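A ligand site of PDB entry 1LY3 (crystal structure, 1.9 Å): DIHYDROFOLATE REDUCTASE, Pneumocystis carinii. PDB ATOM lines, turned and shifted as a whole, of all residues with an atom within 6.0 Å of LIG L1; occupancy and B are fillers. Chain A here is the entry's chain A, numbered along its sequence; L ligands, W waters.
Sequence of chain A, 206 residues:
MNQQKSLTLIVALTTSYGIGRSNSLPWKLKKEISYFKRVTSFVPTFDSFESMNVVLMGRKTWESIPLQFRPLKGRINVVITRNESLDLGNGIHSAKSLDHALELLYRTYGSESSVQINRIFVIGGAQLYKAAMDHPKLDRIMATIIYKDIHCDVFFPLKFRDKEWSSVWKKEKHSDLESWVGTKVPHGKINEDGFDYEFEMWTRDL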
ATOM      1  N   ILE A  10      -5.962 -11.025  24.366  1.00  0.00           N
ATOM      2  CA  ILE A  10      -7.224 -11.701  24.856  1.00  0.00           C
ATOM      3  C   ILE A  10      -6.820 -12.134  26.258  1.00  0.00           C
ATOM      4  O   ILE A  10      -5.778 -12.693  26.501  1.00  0.00           O
ATOM      5  CB  ILE A  10      -7.789 -12.787  23.907  1.00  0.00           C
ATOM      6  CG1 ILE A  10      -9.018 -13.467  24.586  1.00  0.00           C
ATOM      7  CG2 ILE A  10      -6.741 -13.848  23.517  1.00  0.00           C
ATOM      8  CD1 ILE A  10      -9.959 -14.200  23.527  1.00  0.00           C
ATOM      9  N   VAL A  11      -7.700 -11.756  27.198  1.00  0.00           N
ATOM     10  CA  VAL A  11      -7.619 -11.958  28.616  1.00  0.00           C
ATOM     11  C   VAL A  11      -8.945 -12.126  29.371  1.00  0.00           C
ATOM     12  O   VAL A  11     -10.010 -11.614  28.962  1.00  0.00           O
ATOM     13  CB  VAL A  11      -6.882 -10.698  29.188  1.00  0.00           C
ATOM     14  CG1 VAL A  11      -7.570  -9.392  28.921  1.00  0.00           C
ATOM     15  CG2 VAL A  11      -6.466 -11.019  30.590  1.00  0.00           C
ATOM     16  N   ALA A  12      -8.794 -12.854  30.472  1.00  0.00           N
ATOM     17  CA  ALA A  12      -9.893 -13.111  31.402  1.00  0.00           C
ATOM     18  C   ALA A  12      -9.352 -12.562  32.719  1.00  0.00           C
ATOM     19  O   ALA A  12      -8.265 -13.019  33.121  1.00  0.00           O
ATOM     20  CB  ALA A  12     -10.395 -14.516  31.629  1.00  0.00           C
ATOM     21  N   ASN A  23       0.649 -20.166  38.917  1.00  0.00           N
ATOM     22  CA  ASN A  23       0.833 -20.525  37.506  1.00  0.00           C
ATOM     23  C   ASN A  23      -0.320 -21.296  36.869  1.00  0.00           C
ATOM     24  O   ASN A  23      -0.317 -22.149  35.925  1.00  0.00           O
ATOM     25  CB  ASN A  23       2.272 -20.963  37.183  1.00  0.00           C
ATOM     26  CG  ASN A  23       2.522 -20.863  35.676  1.00  0.00           C
ATOM     27  OD1 ASN A  23       3.042 -21.786  35.017  1.00  0.00           O
ATOM     28  ND2 ASN A  23       2.100 -19.723  35.118  1.00  0.00           N
ATOM     29  N   SER A  24      -1.508 -20.922  37.352  1.00  0.00           N
ATOM     30  CA  SER A  24      -2.776 -21.478  36.811  1.00  0.00           C
ATOM     31  C   SER A  24      -3.878 -20.451  36.966  1.00  0.00           C
ATOM     32  O   SER A  24      -3.659 -19.343  37.463  1.00  0.00           O
ATOM     33  CB  SER A  24      -3.147 -22.860  37.357  1.00  0.00           C
ATOM     34  OG  SER A  24      -2.327 -23.033  38.538  1.00  0.00           O
ATOM     35  N   LEU A  25      -5.069 -20.885  36.566  1.00  0.00           N
ATOM     36  CA  LEU A  25      -6.303 -20.101  36.610  1.00  0.00           C
ATOM     37  C   LEU A  25      -7.111 -20.536  37.836  1.00  0.00           C
ATOM     38  O   LEU A  25      -7.621 -21.663  38.011  1.00  0.00           O
ATOM     39  CB  LEU A  25      -7.061 -20.166  35.307  1.00  0.00           C
ATOM     40  CG  LEU A  25      -6.477 -19.601  34.036  1.00  0.00           C
ATOM     41  CD1 LEU A  25      -7.310 -20.015  32.808  1.00  0.00           C
ATOM     42  CD2 LEU A  25      -6.541 -18.071  34.143  1.00  0.00           C
ATOM     43  N   GLU A  32     -16.072 -20.131  29.322  1.00  0.00           N
ATOM     44  CA  GLU A  32     -15.099 -19.031  29.162  1.00  0.00           C
ATOM     45  C   GLU A  32     -13.998 -19.614  28.241  1.00  0.00           C
ATOM     46  O   GLU A  32     -13.650 -18.927  27.247  1.00  0.00           O
ATOM     47  CB  GLU A  32     -14.561 -18.372  30.407  1.00  0.00           C
ATOM     48  CG  GLU A  32     -14.048 -16.931  30.214  1.00  0.00           C
ATOM     49  CD  GLU A  32     -12.784 -16.781  29.402  1.00  0.00           C
ATOM     50  OE1 GLU A  32     -11.902 -17.645  29.612  1.00  0.00           O
ATOM     51  OE2 GLU A  32     -12.796 -15.792  28.622  1.00  0.00           O
ATOM     52  N   ILE A  33     -13.593 -20.841  28.478  1.00  0.00           N
ATOM     53  CA  ILE A  33     -12.624 -21.594  27.650  1.00  0.00           C
ATOM     54  C   ILE A  33     -13.163 -21.805  26.219  1.00  0.00           C
ATOM     55  O   ILE A  33     -12.452 -21.572  25.193  1.00  0.00           O
ATOM     56  CB  ILE A  33     -12.195 -22.868  28.451  1.00  0.00           C
ATOM     57  CG1 ILE A  33     -11.248 -22.547  29.631  1.00  0.00           C
ATOM     58  CG2 ILE A  33     -11.707 -23.978  27.492  1.00  0.00           C
ATOM     59  CD1 ILE A  33      -9.881 -21.954  29.254  1.00  0.00           C
ATOM     60  N   TYR A  35     -15.330 -19.809  24.732  1.00  0.00           N
ATOM     61  CA  TYR A  35     -15.326 -18.529  23.990  1.00  0.00           C
ATOM     62  C   TYR A  35     -13.860 -18.326  23.497  1.00  0.00           C
ATOM     63  O   TYR A  35     -13.678 -17.950  22.305  1.00  0.00           O
ATOM     64  CB  TYR A  35     -15.801 -17.430  24.938  1.00  0.00           C
ATOM     65  CG  TYR A  35     -15.551 -16.013  24.488  1.00  0.00           C
ATOM     66  CD1 TYR A  35     -16.428 -15.429  23.563  1.00  0.00           C
ATOM     67  CD2 TYR A  35     -14.508 -15.239  24.957  1.00  0.00           C
ATOM     68  CE1 TYR A  35     -16.256 -14.124  23.106  1.00  0.00           C
ATOM     69  CE2 TYR A  35     -14.330 -13.922  24.569  1.00  0.00           C
ATOM     70  CZ  TYR A  35     -15.176 -13.382  23.630  1.00  0.00           C
ATOM     71  OH  TYR A  35     -14.977 -12.097  23.189  1.00  0.00           O
ATOM     72  N   PHE A  36     -12.882 -18.465  24.344  1.00  0.00           N
ATOM     73  CA  PHE A  36     -11.461 -18.331  23.954  1.00  0.00           C
ATOM     74  C   PHE A  36     -11.134 -19.095  22.694  1.00  0.00           C
ATOM     75  O   PHE A  36     -10.660 -18.559  21.647  1.00  0.00           O
ATOM     76  CB  PHE A  36     -10.617 -18.762  25.134  1.00  0.00           C
ATOM     77  CG  PHE A  36      -9.140 -18.850  24.872  1.00  0.00           C
ATOM     78  CD1 PHE A  36      -8.426 -17.652  24.728  1.00  0.00           C
ATOM     79  CD2 PHE A  36      -8.518 -20.084  24.755  1.00  0.00           C
ATOM     80  CE1 PHE A  36      -7.044 -17.725  24.541  1.00  0.00           C
ATOM     81  CE2 PHE A  36      -7.136 -20.157  24.531  1.00  0.00           C
ATOM     82  CZ  PHE A  36      -6.409 -18.941  24.459  1.00  0.00           C
ATOM     83  N   THR A  61       2.913 -19.353  30.479  1.00  0.00           N
ATOM     84  CA  THR A  61       1.556 -19.703  30.021  1.00  0.00           C
ATOM     85  C   THR A  61       1.627 -21.015  29.262  1.00  0.00           C
ATOM     86  O   THR A  61       0.668 -21.795  29.393  1.00  0.00           O
ATOM     87  CB  THR A  61       0.865 -18.558  29.190  1.00  0.00           C
ATOM     88  OG1 THR A  61       0.890 -17.505  30.216  1.00  0.00           O
ATOM     89  CG2 THR A  61      -0.500 -18.903  28.699  1.00  0.00           C
ATOM     90  N   SER A  64       1.347 -24.066  31.266  1.00  0.00           N
ATOM     91  CA  SER A  64       0.065 -24.038  31.908  1.00  0.00           C
ATOM     92  C   SER A  64      -1.076 -24.726  31.225  1.00  0.00           C
ATOM     93  O   SER A  64      -2.033 -24.976  31.970  1.00  0.00           O
ATOM     94  CB  SER A  64      -0.442 -22.555  32.056  1.00  0.00           C
ATOM     95  OG  SER A  64       0.237 -22.004  33.172  1.00  0.00           O
ATOM     96  N   ILE A  65      -1.011 -24.912  29.946  1.00  0.00           N
ATOM     97  CA  ILE A  65      -2.079 -25.570  29.176  1.00  0.00           C
ATOM     98  C   ILE A  65      -1.887 -27.084  29.408  1.00  0.00           C
ATOM     99  O   ILE A  65      -0.726 -27.544  29.337  1.00  0.00           O
ATOM    100  CB  ILE A  65      -1.871 -25.173  27.703  1.00  0.00           C
ATOM    101  CG1 ILE A  65      -1.825 -23.602  27.594  1.00  0.00           C
ATOM    102  CG2 ILE A  65      -2.855 -25.863  26.736  1.00  0.00           C
ATOM    103  CD1 ILE A  65      -1.286 -23.285  26.173  1.00  0.00           C
ATOM    104  N   PRO A  66      -2.995 -27.751  29.674  1.00  0.00           N
ATOM    105  CA  PRO A  66      -2.921 -29.201  29.922  1.00  0.00           C
ATOM    106  C   PRO A  66      -2.183 -29.747  28.714  1.00  0.00           C
ATOM    107  O   PRO A  66      -2.412 -29.195  27.648  1.00  0.00           O
ATOM    108  CB  PRO A  66      -4.377 -29.615  30.061  1.00  0.00           C
ATOM    109  CG  PRO A  66      -4.974 -28.381  30.737  1.00  0.00           C
ATOM    110  CD  PRO A  66      -4.330 -27.221  29.944  1.00  0.00           C
ATOM    111  N   PHE A  69      -4.008 -30.252  25.890  1.00  0.00           N
ATOM    112  CA  PHE A  69      -4.507 -29.123  25.069  1.00  0.00           C
ATOM    113  C   PHE A  69      -3.376 -28.278  24.483  1.00  0.00           C
ATOM    114  O   PHE A  69      -3.631 -27.301  23.750  1.00  0.00           O
ATOM    115  CB  PHE A  69      -5.396 -28.224  25.928  1.00  0.00           C
ATOM    116  CG  PHE A  69      -6.495 -29.025  26.586  1.00  0.00           C
ATOM    117  CD1 PHE A  69      -7.536 -29.525  25.808  1.00  0.00           C
ATOM    118  CD2 PHE A  69      -6.439 -29.276  27.963  1.00  0.00           C
ATOM    119  CE1 PHE A  69      -8.542 -30.294  26.400  1.00  0.00           C
ATOM    120  CE2 PHE A  69      -7.446 -30.045  28.555  1.00  0.00           C
ATOM    121  CZ  PHE A  69      -8.494 -30.551  27.775  1.00  0.00           C
ATOM    122  N   LEU A  72      -2.343 -25.458  20.900  1.00  0.00           N
ATOM    123  CA  LEU A  72      -3.721 -25.098  20.623  1.00  0.00           C
ATOM    124  C   LEU A  72      -3.909 -25.485  19.195  1.00  0.00           C
ATOM    125  O   LEU A  72      -3.115 -25.094  18.358  1.00  0.00           O
ATOM    126  CB  LEU A  72      -3.956 -23.643  21.051  1.00  0.00           C
ATOM    127  CG  LEU A  72      -3.622 -23.363  22.500  1.00  0.00           C
ATOM    128  CD1 LEU A  72      -3.975 -21.867  22.802  1.00  0.00           C
ATOM    129  CD2 LEU A  72      -4.370 -24.261  23.468  1.00  0.00           C
ATOM    130  N   VAL A 122      -2.414 -12.130  21.348  1.00  0.00           N
ATOM    131  CA  VAL A 122      -1.475 -12.303  22.508  1.00  0.00           C
ATOM    132  C   VAL A 122      -2.379 -12.966  23.561  1.00  0.00           C
ATOM    133  O   VAL A 122      -3.426 -12.329  24.003  1.00  0.00           O
ATOM    134  CB  VAL A 122      -0.799 -11.001  22.951  1.00  0.00           C
ATOM    135  CG1 VAL A 122       0.110 -11.154  24.184  1.00  0.00           C
ATOM    136  CG2 VAL A 122      -0.105 -10.264  21.795  1.00  0.00           C
ATOM    137  N   ILE A 123      -2.047 -14.149  24.014  1.00  0.00           N
ATOM    138  CA  ILE A 123      -2.897 -14.859  24.993  1.00  0.00           C
ATOM    139  C   ILE A 123      -2.335 -14.970  26.391  1.00  0.00           C
ATOM    140  O   ILE A 123      -2.982 -15.643  27.214  1.00  0.00           O
ATOM    141  CB  ILE A 123      -3.395 -16.225  24.405  1.00  0.00           C
ATOM    142  CG1 ILE A 123      -2.219 -17.206  24.514  1.00  0.00           C
ATOM    143  CG2 ILE A 123      -4.029 -16.010  22.988  1.00  0.00           C
ATOM    144  CD1 ILE A 123      -2.556 -18.726  24.136  1.00  0.00           C
ATOM    145  N   GLY A 124      -1.218 -14.287  26.687  1.00  0.00           N
ATOM    146  CA  GLY A 124      -0.696 -14.239  28.069  1.00  0.00           C
ATOM    147  C   GLY A 124       0.724 -14.664  28.276  1.00  0.00           C
ATOM    148  O   GLY A 124       1.339 -15.113  27.285  1.00  0.00           O
ATOM    149  N   TYR A 129       2.003  -9.738  28.311  1.00  0.00           N
ATOM    150  CA  TYR A 129       0.959  -8.710  28.262  1.00  0.00           C
ATOM    151  C   TYR A 129       1.624  -7.327  28.451  1.00  0.00           C
ATOM    152  O   TYR A 129       1.113  -6.415  27.819  1.00  0.00           O
ATOM    153  CB  TYR A 129      -0.162  -8.901  29.320  1.00  0.00           C
ATOM    154  CG  TYR A 129      -1.156 -10.002  29.109  1.00  0.00           C
ATOM    155  CD1 TYR A 129      -1.707 -10.290  27.827  1.00  0.00           C
ATOM    156  CD2 TYR A 129      -1.672 -10.681  30.205  1.00  0.00           C
ATOM    157  CE1 TYR A 129      -2.697 -11.263  27.592  1.00  0.00           C
ATOM    158  CE2 TYR A 129      -2.661 -11.654  30.007  1.00  0.00           C
ATOM    159  CZ  TYR A 129      -3.098 -11.938  28.748  1.00  0.00           C
ATOM    160  OH  TYR A 129      -4.063 -12.967  28.705  1.00  0.00           O
ATOM    161  N   MET A 142      -9.611  -8.156  23.947  1.00  0.00           N
ATOM    162  CA  MET A 142     -10.848  -8.968  24.083  1.00  0.00           C
ATOM    163  C   MET A 142     -10.834  -9.269  25.550  1.00  0.00           C
ATOM    164  O   MET A 142     -10.006 -10.110  25.930  1.00  0.00           O
ATOM    165  CB  MET A 142     -10.907 -10.245  23.209  1.00  0.00           C
ATOM    166  CG  MET A 142     -10.570  -9.911  21.768  1.00  0.00           C
ATOM    167  SD  MET A 142     -11.893  -8.895  21.086  1.00  0.00           S
ATOM    168  CE  MET A 142     -13.203 -10.076  20.755  1.00  0.00           C
ATOM    169  N   ALA A 143     -11.685  -8.656  26.359  1.00  0.00           N
ATOM    170  CA  ALA A 143     -11.588  -9.002  27.821  1.00  0.00           C
ATOM    171  C   ALA A 143     -12.751  -9.762  28.400  1.00  0.00           C
ATOM    172  O   ALA A 143     -13.893  -9.433  28.124  1.00  0.00           O
ATOM    173  CB  ALA A 143     -11.409  -7.632  28.551  1.00  0.00           C
ATOM    174  N   THR A 144     -12.477 -10.663  29.320  1.00  0.00           N
ATOM    175  CA  THR A 144     -13.605 -11.345  29.995  1.00  0.00           C
ATOM    176  C   THR A 144     -13.537 -10.789  31.412  1.00  0.00           C
ATOM    177  O   THR A 144     -12.547 -11.100  32.033  1.00  0.00           O
ATOM    178  CB  THR A 144     -13.535 -12.928  29.999  1.00  0.00           C
ATOM    179  OG1 THR A 144     -13.630 -13.191  28.584  1.00  0.00           O
ATOM    180  CG2 THR A 144     -14.675 -13.514  30.896  1.00  0.00           C
HETATM  181  C1  LIG L   1      -9.273 -15.693  27.958  1.00  0.00           C
HETATM  182  C2  LIG L   1      -6.917 -16.098  27.591  1.00  0.00           C
HETATM  183  C3  LIG L   1      -7.058 -17.378  28.170  1.00  0.00           C
HETATM  184  C4  LIG L   1      -5.970 -18.251  28.291  1.00  0.00           C
HETATM  185  C5  LIG L   1      -6.158 -19.507  28.900  1.00  0.00           C
HETATM  186  C6  LIG L   1      -7.422 -19.870  29.348  1.00  0.00           C
HETATM  187  C7  LIG L   1      -8.334 -17.789  28.613  1.00  0.00           C
HETATM  188  C8  LIG L   1      -4.530 -23.149  33.055  1.00  0.00           C
HETATM  189  C9  LIG L   1      -4.694 -21.190  30.014  1.00  0.00           C
HETATM  190  C10 LIG L   1      -4.137 -19.957  27.791  1.00  0.00           C
HETATM  191  C11 LIG L   1      -5.521 -22.473  29.791  1.00  0.00           C
HETATM  192  C12 LIG L   1      -5.859 -23.246  30.897  1.00  0.00           C
HETATM  193  C13 LIG L   1      -6.574 -24.430  30.698  1.00  0.00           C
HETATM  194  C14 LIG L   1      -6.916 -24.845  29.421  1.00  0.00           C
HETATM  195  C15 LIG L   1      -6.539 -24.074  28.328  1.00  0.00           C
HETATM  196  C16 LIG L   1      -7.376 -25.809  26.732  1.00  0.00           C
HETATM  197  C17 LIG L   1      -5.825 -22.901  28.518  1.00  0.00           C
HETATM  198  N1  LIG L   1      -9.420 -16.944  28.521  1.00  0.00           N
HETATM  199  N2  LIG L   1     -10.389 -14.851  27.797  1.00  0.00           N
HETATM  200  N3  LIG L   1      -8.008 -15.283  27.467  1.00  0.00           N
HETATM  201  N4  LIG L   1      -5.690 -15.570  27.143  1.00  0.00           N
HETATM  202  C18 LIG L   1      -8.533 -19.051  29.233  1.00  0.00           C
HETATM  203  O1  LIG L   1      -5.586 -22.878  32.173  1.00  0.00           O
HETATM  204  O2  LIG L   1      -6.933 -24.528  27.062  1.00  0.00           O
HETATM  205  N5  LIG L   1      -4.982 -20.273  28.934  1.00  0.00           N
HETATM  206  P1  LG2 L   2       4.267 -15.338  31.042  1.00  0.00           P
HETATM  207  O1  LG2 L   2       3.405 -16.431  30.398  1.00  0.00           O
HETATM  208  O2  LG2 L   2       4.259 -14.072  30.369  1.00  0.00           O
HETATM  209  O3  LG2 L   2       5.763 -16.126  30.933  1.00  0.00           O
HETATM  210  C1  LG2 L   2       6.931 -15.294  31.295  1.00  0.00           C
HETATM  211  C2  LG2 L   2       8.058 -15.997  30.483  1.00  0.00           C
HETATM  212  O4  LG2 L   2       7.801 -15.801  29.262  1.00  0.00           O
HETATM  213  C3  LG2 L   2       9.405 -15.113  30.756  1.00  0.00           C
HETATM  214  O5  LG2 L   2       9.932 -15.807  32.003  1.00  0.00           O
HETATM  215  C4  LG2 L   2      10.102 -15.489  29.429  1.00  0.00           C
HETATM  216  O6  LG2 L   2      10.486 -16.797  29.188  1.00  0.00           O
HETATM  217  C5  LG2 L   2       8.863 -15.241  28.494  1.00  0.00           C
HETATM  218  N1  LG2 L   2       8.574 -13.845  28.167  1.00  0.00           N
HETATM  219  C6  LG2 L   2       7.385 -13.221  28.451  1.00  0.00           C
HETATM  220  N2  LG2 L   2       7.373 -11.980  28.089  1.00  0.00           N
HETATM  221  C7  LG2 L   2       8.681 -11.860  27.468  1.00  0.00           C
HETATM  222  C8  LG2 L   2       9.443 -10.708  26.751  1.00  0.00           C
HETATM  223  N3  LG2 L   2       8.851  -9.498  26.616  1.00  0.00           N
HETATM  224  N4  LG2 L   2      10.689 -10.949  26.320  1.00  0.00           N
HETATM  225  C9  LG2 L   2      11.146 -12.189  26.521  1.00  0.00           C
HETATM  226  N5  LG2 L   2      10.594 -13.235  27.117  1.00  0.00           N
HETATM  227  C10 LG2 L   2       9.359 -12.981  27.566  1.00  0.00           C
HETATM  228  O7  LG2 L   2       4.050 -15.540  32.593  1.00  0.00           O
HETATM  229  P2  LG2 L   2       3.475 -14.811  33.898  1.00  0.00           P
HETATM  230  O8  LG2 L   2       3.657 -13.431  33.893  1.00  0.00           O
HETATM  231  O9  LG2 L   2       4.002 -15.440  35.102  1.00  0.00           O
HETATM  232  O10 LG2 L   2       1.925 -15.199  33.844  1.00  0.00           O
HETATM  233  C11 LG2 L   2       1.543 -16.551  33.874  1.00  0.00           C
HETATM  234  C12 LG2 L   2       0.277 -16.464  34.716  1.00  0.00           C
HETATM  235  O11 LG2 L   2      -0.761 -15.803  33.853  1.00  0.00           O
HETATM  236  C13 LG2 L   2      -0.190 -17.918  35.050  1.00  0.00           C
HETATM  237  O12 LG2 L   2      -0.771 -17.856  36.374  1.00  0.00           O
HETATM  238  C14 LG2 L   2      -1.261 -18.123  33.923  1.00  0.00           C
HETATM  239  O13 LG2 L   2      -2.181 -18.982  34.540  1.00  0.00           O
HETATM  240  C15 LG2 L   2      -1.869 -16.741  33.827  1.00  0.00           C
HETATM  241  N6  LG2 L   2      -2.691 -16.371  32.585  1.00  0.00           N
HETATM  242  C16 LG2 L   2      -4.011 -15.891  32.702  1.00  0.00           C
HETATM  243  C17 LG2 L   2      -4.669 -15.559  31.564  1.00  0.00           C
HETATM  244  C18 LG2 L   2      -6.062 -15.023  31.704  1.00  0.00           C
HETATM  245  O14 LG2 L   2      -6.504 -14.757  30.634  1.00  0.00           O
HETATM  246  N7  LG2 L   2      -6.524 -14.962  33.007  1.00  0.00           N
HETATM  247  C19 LG2 L   2      -4.117 -15.704  30.139  1.00  0.00           C
HETATM  248  C20 LG2 L   2      -2.738 -16.283  30.223  1.00  0.00           C
HETATM  249  C21 LG2 L   2      -2.096 -16.571  31.335  1.00  0.00           C
HETATM  250  P3  LG2 L   2      12.040 -17.374  29.753  1.00  0.00           P
HETATM  251  O15 LG2 L   2      12.881 -16.457  28.860  1.00  0.00           O
HETATM  252  O16 LG2 L   2      11.930 -18.769  29.438  1.00  0.00           O
HETATM  253  O17 LG2 L   2      12.214 -16.773  31.109  1.00  0.00           O
HETATM  254  O   HOH W   1      -3.240 -20.277  32.301  1.00  0.00           O
HETATM  255  O   HOH W   2     -12.126 -12.206  26.435  1.00  0.00           O
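The backbone carbonyl oxygen (O) of Ile 123 is in hydrogen-bond range of a nitrogen (N4) of LIG L1. The side-chain hydroxyl (OG1) of Thr 61 lies within hydrogen-bond range of an oxygen (O1) of LG2 L2 (2.7 Å). An oxygen (O14) of LG2 L2 sits at hydrogen-bond distance from the backbone NH (N) of Ala 12 (3.0 Å). The backbone NH of Ser 24 sits at hydrogen-bond distance from an oxygen (O12) of LG2 L2, 3.3 Å away. A nitrogen (N4) of LIG L1 lies within hydrogen-bond range of the side-chain hydroxyl (OH) of Tyr 129. The backbone carbonyl oxygen (O) of Ser 24 lies within hydrogen-bond range of an oxygen (O13) of LG2 L2 (3.3 Å). A nitrogen (N2) of LIG L1 sits at hydrogen-bond distance from the side-chain carboxylate (OE2) of Glu 32 (2.7 Å). O1 of LG2 L2 sits at hydrogen-bond distance from N of Thr 61, at 3.0 Å. O of Ala 12 lies within hydrogen-bond range of N7 of LG2 L2 (2.6 Å). The backbone carbonyl oxygen of Val 11 is in hydrogen-bond range of a nitrogen (N2) of LIG L1 (3.5 Å). O of Ile 10 sits at hydrogen-bond distance from N4 of LIG L1 (2.9 Å).
OH of Tyr 129 is in hydrogen-bond range of O of Ile 10 (2.8 Å). O of Val 122 sits at hydrogen-bond distance from N of Ile 10, at 2.9 Å. The backbone carbonyl oxygen (O) of Asn 23 is in hydrogen-bond range of the side-chain hydroxyl (OG) of Ser 64. The backbone NH (N) of Val 11 is in hydrogen-bond range of the backbone carbonyl oxygen (O) of Met 142, 3.1 Å away. The backbone carbonyl oxygen (O) of Val 11 is in hydrogen-bond range of the backbone NH (N) of Thr 144 (2.7 Å). The side-chain hydroxyl of Tyr 129 sits at hydrogen-bond distance from the backbone carbonyl oxygen of Ile 123, 3.2 Å away. OE2 of Glu 32 is in hydrogen-bond range of OG1 of Thr 144, at 2.7 Å.
Ala 12 touches LIG L1 (N to N2, 3.7 Å). CD1 of Leu 25 touches O1 of LIG L1 (3.4 Å). Ile 33 touches LIG L1 (CD1 to C18, 3.2 Å). Phe 36 touches LIG L1. Thr 61 touches LIG L1 (CG2 to C10, 3.9 Å). Ser 64 touches LIG L1 (O to C8, 3.3 Å). CD of Pro 66 touches C14 of LIG L1 (3.6 Å). Phe 69 touches LIG L1. OG1 of Thr 144 touches N2 of LIG L1, 3.7 Å away. 14 residues have an atom within 4 Å of LIG L1: Ile 10, Val 11, Ala 12, Leu 25, Glu 32, Ile 33, Phe 36, Thr 61, Ser 64, Pro 66, Phe 69, Ile 123, Tyr 129 and Thr 144.
Water W2 lies within hydrogen-bond range of the side-chain hydroxyl of Thr 144 (2.8 Å), the backbone carbonyl oxygen of Met 142 (3.0 Å), the backbone carbonyl oxygen of Val 11 (3.3 Å) and a nitrogen (N2) of LIG L1 (3.4 Å).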
